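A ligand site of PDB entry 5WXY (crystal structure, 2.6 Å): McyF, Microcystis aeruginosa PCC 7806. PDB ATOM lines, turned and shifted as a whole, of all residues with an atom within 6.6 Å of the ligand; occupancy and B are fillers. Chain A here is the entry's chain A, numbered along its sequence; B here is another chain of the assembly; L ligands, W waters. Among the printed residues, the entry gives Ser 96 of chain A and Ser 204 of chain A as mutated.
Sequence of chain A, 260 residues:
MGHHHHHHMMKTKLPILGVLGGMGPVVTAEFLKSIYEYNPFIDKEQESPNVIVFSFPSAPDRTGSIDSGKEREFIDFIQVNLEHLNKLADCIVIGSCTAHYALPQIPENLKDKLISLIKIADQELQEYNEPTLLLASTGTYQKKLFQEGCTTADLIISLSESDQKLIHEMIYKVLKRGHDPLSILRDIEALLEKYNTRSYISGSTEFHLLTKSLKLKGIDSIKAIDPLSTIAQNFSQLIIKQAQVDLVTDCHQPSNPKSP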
ATOM      1  N   GLY A  22       3.883  38.044 -16.979  1.00  0.00           N
ATOM      2  CA  GLY A  22       5.016  38.117 -16.081  1.00  0.00           C
ATOM      3  C   GLY A  22       5.130  36.873 -15.214  1.00  0.00           C
ATOM      4  O   GLY A  22       5.806  36.897 -14.207  1.00  0.00           O
ATOM      5  N   MET A  23       4.502  35.764 -15.631  1.00  0.00           N
ATOM      6  CA  MET A  23       4.392  34.555 -14.812  1.00  0.00           C
ATOM      7  C   MET A  23       4.710  33.300 -15.638  1.00  0.00           C
ATOM      8  O   MET A  23       3.850  32.456 -15.815  1.00  0.00           O
ATOM      9  CB  MET A  23       2.986  34.447 -14.213  1.00  0.00           C
ATOM     10  CG  MET A  23       2.587  35.629 -13.346  1.00  0.00           C
ATOM     11  SD  MET A  23       0.931  35.494 -12.645  1.00  0.00           S
ATOM     12  CE  MET A  23      -0.083  35.791 -14.076  1.00  0.00           C
ATOM     13  N   GLY A  24       5.941  33.151 -16.148  1.00  0.00           N
ATOM     14  CA  GLY A  24       7.033  34.108 -15.991  1.00  0.00           C
ATOM     15  C   GLY A  24       7.179  35.130 -17.110  1.00  0.00           C
ATOM     16  O   GLY A  24       6.450  35.075 -18.112  1.00  0.00           O
ATOM     17  N   VAL A  27       8.473  33.738 -20.910  1.00  0.00           N
ATOM     18  CA  VAL A  27       7.410  33.141 -21.718  1.00  0.00           C
ATOM     19  C   VAL A  27       6.347  34.156 -22.143  1.00  0.00           C
ATOM     20  O   VAL A  27       5.785  34.033 -23.227  1.00  0.00           O
ATOM     21  CB  VAL A  27       6.784  31.907 -21.037  1.00  0.00           C
ATOM     22  CG1 VAL A  27       5.964  32.272 -19.801  1.00  0.00           C
ATOM     23  CG2 VAL A  27       5.934  31.133 -22.028  1.00  0.00           C
ATOM     24  N   ASP A  61       5.164  34.154  -6.430  1.00  0.00           N
ATOM     25  CA  ASP A  61       5.243  32.820  -7.071  1.00  0.00           C
ATOM     26  C   ASP A  61       3.958  32.031  -6.809  1.00  0.00           C
ATOM     27  O   ASP A  61       3.398  32.095  -5.706  1.00  0.00           O
ATOM     28  CB  ASP A  61       6.470  32.018  -6.611  1.00  0.00           C
ATOM     29  CG  ASP A  61       6.688  30.731  -7.435  1.00  0.00           C
ATOM     30  OD1 ASP A  61       6.513  30.755  -8.683  1.00  0.00           O
ATOM     31  OD2 ASP A  61       7.046  29.687  -6.855  1.00  0.00           O
ATOM     32  N   ARG A  62       3.487  31.332  -7.839  1.00  0.00           N
ATOM     33  CA  ARG A  62       2.144  30.732  -7.836  1.00  0.00           C
ATOM     34  C   ARG A  62       2.120  29.465  -6.990  1.00  0.00           C
ATOM     35  O   ARG A  62       1.245  29.314  -6.122  1.00  0.00           O
ATOM     36  CB  ARG A  62       1.680  30.428  -9.268  1.00  0.00           C
ATOM     37  CG  ARG A  62       1.094  31.608 -10.050  1.00  0.00           C
ATOM     38  CD  ARG A  62       1.984  32.849 -10.091  1.00  0.00           C
ATOM     39  NE  ARG A  62       3.244  32.659 -10.832  1.00  0.00           N
ATOM     40  CZ  ARG A  62       4.236  33.551 -10.871  1.00  0.00           C
ATOM     41  NH1 ARG A  62       5.327  33.295 -11.605  1.00  0.00           N
ATOM     42  NH2 ARG A  62       4.165  34.706 -10.210  1.00  0.00           N
ATOM     43  N   THR A  63       3.078  28.573  -7.248  1.00  0.00           N
ATOM     44  CA  THR A  63       3.286  27.383  -6.419  1.00  0.00           C
ATOM     45  C   THR A  63       3.695  27.800  -4.993  1.00  0.00           C
ATOM     46  O   THR A  63       3.187  27.241  -4.030  1.00  0.00           O
ATOM     47  CB  THR A  63       4.343  26.433  -7.047  1.00  0.00           C
ATOM     48  OG1 THR A  63       3.833  25.925  -8.289  1.00  0.00           O
ATOM     49  CG2 THR A  63       4.669  25.259  -6.132  1.00  0.00           C
ATOM     50  N   PHE A  74      -1.916  36.580  -3.437  1.00  0.00           N
ATOM     51  CA  PHE A  74      -1.916  36.277  -4.865  1.00  0.00           C
ATOM     52  C   PHE A  74      -3.257  36.518  -5.570  1.00  0.00           C
ATOM     53  O   PHE A  74      -3.280  37.000  -6.694  1.00  0.00           O
ATOM     54  CB  PHE A  74      -1.462  34.839  -5.152  1.00  0.00           C
ATOM     55  CG  PHE A  74      -1.355  34.549  -6.612  1.00  0.00           C
ATOM     56  CD1 PHE A  74      -0.336  35.136  -7.360  1.00  0.00           C
ATOM     57  CD2 PHE A  74      -2.305  33.770  -7.265  1.00  0.00           C
ATOM     58  CE1 PHE A  74      -0.249  34.917  -8.722  1.00  0.00           C
ATOM     59  CE2 PHE A  74      -2.218  33.550  -8.627  1.00  0.00           C
ATOM     60  CZ  PHE A  74      -1.191  34.131  -9.355  1.00  0.00           C
ATOM     61  N   GLY A  95      -1.358  34.499 -18.288  1.00  0.00           N
ATOM     62  CA  GLY A  95      -0.231  33.760 -18.860  1.00  0.00           C
ATOM     63  C   GLY A  95       0.418  32.749 -17.938  1.00  0.00           C
ATOM     64  O   GLY A  95       1.628  32.524 -18.012  1.00  0.00           O
ATOM     65  N   SER A  96      -0.399  32.127 -17.088  1.00  0.00           N
ATOM     66  CA  SER A  96       0.046  31.076 -16.197  1.00  0.00           C
ATOM     67  C   SER A  96      -1.132  30.135 -15.977  1.00  0.00           C
ATOM     68  O   SER A  96      -2.227  30.583 -15.644  1.00  0.00           O
ATOM     69  CB  SER A  96       0.511  31.657 -14.852  1.00  0.00           C
ATOM     70  OG  SER A  96       0.443  30.710 -13.798  1.00  0.00           O
ATOM     71  N   CYS A  97      -0.904  28.832 -16.156  1.00  0.00           N
ATOM     72  CA  CYS A  97      -1.911  27.837 -15.835  1.00  0.00           C
ATOM     73  C   CYS A  97      -2.139  27.781 -14.332  1.00  0.00           C
ATOM     74  O   CYS A  97      -3.271  27.958 -13.886  1.00  0.00           O
ATOM     75  CB  CYS A  97      -1.506  26.475 -16.354  1.00  0.00           C
ATOM     76  SG  CYS A  97      -1.594  26.375 -18.146  1.00  0.00           S
ATOM     77  N   THR A  98      -1.076  27.568 -13.546  1.00  0.00           N
ATOM     78  CA  THR A  98      -1.181  27.542 -12.075  1.00  0.00           C
ATOM     79  C   THR A  98      -2.035  28.696 -11.541  1.00  0.00           C
ATOM     80  O   THR A  98      -2.935  28.473 -10.748  1.00  0.00           O
ATOM     81  CB  THR A  98       0.182  27.577 -11.359  1.00  0.00           C
ATOM     82  OG1 THR A  98       1.097  26.667 -11.984  1.00  0.00           O
ATOM     83  CG2 THR A  98       0.040  27.164  -9.891  1.00  0.00           C
ATOM     84  N   ALA A  99      -1.794  29.913 -12.045  1.00  0.00           N
ATOM     85  CA  ALA A  99      -2.523  31.138 -11.635  1.00  0.00           C
ATOM     86  C   ALA A  99      -4.036  31.054 -11.746  1.00  0.00           C
ATOM     87  O   ALA A  99      -4.759  31.808 -11.078  1.00  0.00           O
ATOM     88  CB  ALA A  99      -2.036  32.340 -12.435  1.00  0.00           C
ATOM     89  N   LEU A 117      -6.853  29.085 -20.184  1.00  0.00           N
ATOM     90  CA  LEU A 117      -5.825  28.159 -20.666  1.00  0.00           C
ATOM     91  C   LEU A 117      -6.189  26.691 -20.437  1.00  0.00           C
ATOM     92  O   LEU A 117      -5.850  25.849 -21.275  1.00  0.00           O
ATOM     93  CB  LEU A 117      -4.483  28.444 -19.991  1.00  0.00           C
ATOM     94  CG  LEU A 117      -3.827  29.813 -20.231  1.00  0.00           C
ATOM     95  CD1 LEU A 117      -2.408  29.773 -19.687  1.00  0.00           C
ATOM     96  CD2 LEU A 117      -3.840  30.249 -21.696  1.00  0.00           C
ATOM     97  N   ALA A 136       3.743  19.865 -15.685  1.00  0.00           N
ATOM     98  CA  ALA A 136       3.482  20.896 -14.646  1.00  0.00           C
ATOM     99  C   ALA A 136       4.387  20.407 -13.481  1.00  0.00           C
ATOM    100  O   ALA A 136       4.595  19.196 -13.414  1.00  0.00           O
ATOM    101  CB  ALA A 136       2.017  20.884 -14.298  1.00  0.00           C
ATOM    102  N   SER A 137       4.931  21.209 -12.539  1.00  0.00           N
ATOM    103  CA  SER A 137       4.318  22.245 -11.674  1.00  0.00           C
ATOM    104  C   SER A 137       3.501  21.533 -10.579  1.00  0.00           C
ATOM    105  O   SER A 137       2.319  21.216 -10.783  1.00  0.00           O
ATOM    106  CB  SER A 137       3.504  23.326 -12.404  1.00  0.00           C
ATOM    107  OG  SER A 137       3.092  24.329 -11.462  1.00  0.00           O
ATOM    108  N   THR A 140       0.252  23.286  -9.763  1.00  0.00           N
ATOM    109  CA  THR A 140      -0.823  23.003 -10.725  1.00  0.00           C
ATOM    110  C   THR A 140      -1.409  21.632 -10.464  1.00  0.00           C
ATOM    111  O   THR A 140      -2.623  21.448 -10.579  1.00  0.00           O
ATOM    112  CB  THR A 140      -0.291  23.067 -12.182  1.00  0.00           C
ATOM    113  OG1 THR A 140       0.105  24.408 -12.486  1.00  0.00           O
ATOM    114  CG2 THR A 140      -1.335  22.634 -13.192  1.00  0.00           C
ATOM    115  N   ILE A 171      11.581  23.740 -15.446  1.00  0.00           N
ATOM    116  CA  ILE A 171      10.908  25.024 -15.571  1.00  0.00           C
ATOM    117  C   ILE A 171      11.793  26.125 -14.984  1.00  0.00           C
ATOM    118  O   ILE A 171      12.179  27.054 -15.698  1.00  0.00           O
ATOM    119  CB  ILE A 171       9.494  24.999 -14.935  1.00  0.00           C
ATOM    120  CG1 ILE A 171       8.548  24.129 -15.772  1.00  0.00           C
ATOM    121  CG2 ILE A 171       8.911  26.408 -14.825  1.00  0.00           C
ATOM    122  CD1 ILE A 171       7.297  23.696 -15.037  1.00  0.00           C
ATOM    123  N   TYR A 172      12.142  25.986 -13.706  1.00  0.00           N
ATOM    124  CA  TYR A 172      12.829  27.046 -12.966  1.00  0.00           C
ATOM    125  C   TYR A 172      14.317  27.162 -13.302  1.00  0.00           C
ATOM    126  O   TYR A 172      14.818  28.274 -13.403  1.00  0.00           O
ATOM    127  CB  TYR A 172      12.593  26.902 -11.451  1.00  0.00           C
ATOM    128  CG  TYR A 172      11.205  27.366 -11.024  1.00  0.00           C
ATOM    129  CD1 TYR A 172      10.068  26.633 -11.378  1.00  0.00           C
ATOM    130  CD2 TYR A 172      11.025  28.526 -10.269  1.00  0.00           C
ATOM    131  CE1 TYR A 172       8.786  27.053 -11.002  1.00  0.00           C
ATOM    132  CE2 TYR A 172       9.743  28.946  -9.893  1.00  0.00           C
ATOM    133  CZ  TYR A 172       8.643  28.199 -10.261  1.00  0.00           C
ATOM    134  OH  TYR A 172       7.358  28.598  -9.906  1.00  0.00           O
ATOM    135  N   LYS A 176      12.524  29.347 -17.280  1.00  0.00           N
ATOM    136  CA  LYS A 176      12.292  30.696 -16.752  1.00  0.00           C
ATOM    137  C   LYS A 176      13.547  31.586 -16.837  1.00  0.00           C
ATOM    138  O   LYS A 176      13.426  32.809 -16.858  1.00  0.00           O
ATOM    139  CB  LYS A 176      11.797  30.647 -15.301  1.00  0.00           C
ATOM    140  CG  LYS A 176      10.377  30.112 -15.145  1.00  0.00           C
ATOM    141  CD  LYS A 176       9.958  30.068 -13.676  1.00  0.00           C
ATOM    142  CE  LYS A 176       8.461  29.843 -13.500  1.00  0.00           C
ATOM    143  NZ  LYS A 176       7.535  30.951 -13.860  1.00  0.00           N
ATOM    144  N   SER A 202       1.114  21.441 -22.219  1.00  0.00           N
ATOM    145  CA  SER A 202       1.825  22.492 -21.496  1.00  0.00           C
ATOM    146  C   SER A 202       1.009  22.907 -20.255  1.00  0.00           C
ATOM    147  O   SER A 202       0.309  23.922 -20.275  1.00  0.00           O
ATOM    148  CB  SER A 202       2.069  23.693 -22.415  1.00  0.00           C
ATOM    149  OG  SER A 202       2.893  23.328 -23.491  1.00  0.00           O
ATOM    150  N   GLY A 203       1.103  22.109 -19.196  1.00  0.00           N
ATOM    151  CA  GLY A 203       0.453  22.451 -17.923  1.00  0.00           C
ATOM    152  C   GLY A 203       1.110  23.638 -17.234  1.00  0.00           C
ATOM    153  O   GLY A 203       0.494  24.311 -16.438  1.00  0.00           O
ATOM    154  N   SER A 204       2.398  23.832 -17.526  1.00  0.00           N
ATOM    155  CA  SER A 204       3.098  25.076 -17.261  1.00  0.00           C
ATOM    156  C   SER A 204       3.190  25.839 -18.569  1.00  0.00           C
ATOM    157  O   SER A 204       3.506  25.233 -19.608  1.00  0.00           O
ATOM    158  CB  SER A 204       4.496  24.782 -16.732  1.00  0.00           C
ATOM    159  OG  SER A 204       5.307  25.943 -16.745  1.00  0.00           O
ATOM    160  N   THR A 205       2.949  27.159 -18.520  1.00  0.00           N
ATOM    161  CA  THR A 205       3.060  28.000 -19.723  1.00  0.00           C
ATOM    162  C   THR A 205       4.485  28.079 -20.258  1.00  0.00           C
ATOM    163  O   THR A 205       4.661  28.283 -21.458  1.00  0.00           O
ATOM    164  CB  THR A 205       2.490  29.415 -19.535  1.00  0.00           C
ATOM    165  OG1 THR A 205       3.061  30.032 -18.384  1.00  0.00           O
ATOM    166  CG2 THR A 205       0.984  29.369 -19.379  1.00  0.00           C
ATOM    167  N   GLU A 206       5.484  27.872 -19.400  1.00  0.00           N
ATOM    168  CA  GLU A 206       6.871  27.841 -19.873  1.00  0.00           C
ATOM    169  C   GLU A 206       7.141  26.762 -20.927  1.00  0.00           C
ATOM    170  O   GLU A 206       8.143  26.848 -21.635  1.00  0.00           O
ATOM    171  CB  GLU A 206       7.884  27.708 -18.718  1.00  0.00           C
ATOM    172  CG  GLU A 206       8.315  29.038 -18.084  1.00  0.00           C
ATOM    173  CD  GLU A 206       7.295  29.604 -17.114  1.00  0.00           C
ATOM    174  OE1 GLU A 206       7.361  30.820 -16.787  1.00  0.00           O
ATOM    175  OE2 GLU A 206       6.409  28.839 -16.665  1.00  0.00           O
ATOM    176  N   GLU B  45      12.191  35.207 -10.078  1.00  0.00           N
ATOM    177  CA  GLU B  45      11.546  36.037 -11.114  1.00  0.00           C
ATOM    178  C   GLU B  45      11.047  37.370 -10.609  1.00  0.00           C
ATOM    179  O   GLU B  45      10.986  38.330 -11.367  1.00  0.00           O
ATOM    180  CB  GLU B  45      10.332  35.339 -11.713  1.00  0.00           C
ATOM    181  CG  GLU B  45      10.661  34.289 -12.739  1.00  0.00           C
ATOM    182  CD  GLU B  45       9.449  33.558 -13.249  1.00  0.00           C
ATOM    183  OE1 GLU B  45       8.417  33.474 -12.545  1.00  0.00           O
ATOM    184  OE2 GLU B  45       9.554  33.072 -14.378  1.00  0.00           O
HETATM  185  N1  LIG L   1       4.073  29.671 -15.808  1.00  0.00           N
HETATM  186  C1  LIG L   1       3.842  28.452 -14.936  1.00  0.00           C
HETATM  187  C2  LIG L   1       2.406  27.928 -15.032  1.00  0.00           C
HETATM  188  O1  LIG L   1       1.618  28.336 -15.877  1.00  0.00           O
HETATM  189  C3  LIG L   1       4.267  28.713 -13.484  1.00  0.00           C
HETATM  190  C4  LIG L   1       3.997  30.131 -13.033  1.00  0.00           C
HETATM  191  O2  LIG L   1       2.816  30.521 -12.994  1.00  0.00           O
HETATM  192  O3  LIG L   1       4.971  30.846 -12.744  1.00  0.00           O
HETATM  193  O4  LIG L   1       1.998  27.031 -14.303  1.00  0.00           O
HETATM  194  O   HOH W   1       4.531  27.785 -10.201  1.00  0.00           O
HETATM  195  O   HOH W   2       5.380  25.973 -13.446  1.00  0.00           O
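An oxygen (O2) of the ligand is in hydrogen-bond range of the side-chain hydroxyl of Ser 96, at 2.5 Å.
N of Thr 98 is in hydrogen-bond range of O4 of the ligand, 3.2 Å away.
An oxygen (O4) of the ligand sits at hydrogen-bond distance from the side-chain hydroxyl (OG1) of Thr 98.
N of Cys 97 lies within hydrogen-bond range of O1 of the ligand (2.6 Å).
The side-chain carboxylate (OE2) of Glu 206 is in salt-bridge range of a nitrogen (N1) of the ligand.
The guanidinium group (NH1) of Arg 62 lies within salt-bridge range of an oxygen (O3) of the ligand, at 2.7 Å.
The backbone NH (N) of Thr 205 is in hydrogen-bond range of an oxygen (O1) of the ligand (3.2 Å).
OG1 of Thr 205 is in hydrogen-bond range of N1 of the ligand (2.8 Å).
The backbone carbonyl oxygen of Met 23 lies within hydrogen-bond range of a nitrogen (N1) of the ligand.
The side-chain amino group of Lys 176 lies within salt-bridge range of an oxygen (O3) of the ligand.
The backbone NH of Thr 98 lies within hydrogen-bond range of the side-chain hydroxyl of Ser 96, 3.5 Å away.
The side-chain sulfur of Cys 97 lies within hydrogen-bond range of the backbone carbonyl oxygen of Ser 202 (3.8 Å).
The side-chain carboxylate (OE1) of Glu 206 lies within salt-bridge range of the side-chain amino group (NZ) of Lys 176, 2.9 Å away.
N of Gly 24 sits at hydrogen-bond distance from OE1 of Glu 206, 2.8 Å away.
The guanidinium group (NH1) of Arg 62 is in salt-bridge range of the side-chain carboxylate (OE1) of Glu 45 of chain B.
The side-chain amino group (NZ) of Lys 176 is in salt-bridge range of the side-chain carboxylate (OE2) of Glu 45 of chain B, 3.0 Å away.
The backbone carbonyl oxygen (O) of Ile 171 sits at hydrogen-bond distance from the backbone NH (N) of Lys 176, 2.8 Å away.
OG1 of Thr 140 sits at hydrogen-bond distance from OG of Ser 137 (3.2 Å).
Merely in contact with the ligand: Ser 204 (3.4 Å), Thr 140 (3.7 Å), Gly 203 (3.8 Å) and Gly 24 (3.96 Å).
Water W2 bridges OG of Ser 204 (3.3 Å) and OG of Ser 137 (3.4 Å).
Water W1 lies within hydrogen-bond range of the side-chain hydroxyl (OG1) of Thr 63 (2.8 Å) and the side-chain hydroxyl (OH) of Tyr 172 (3.0 Å).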
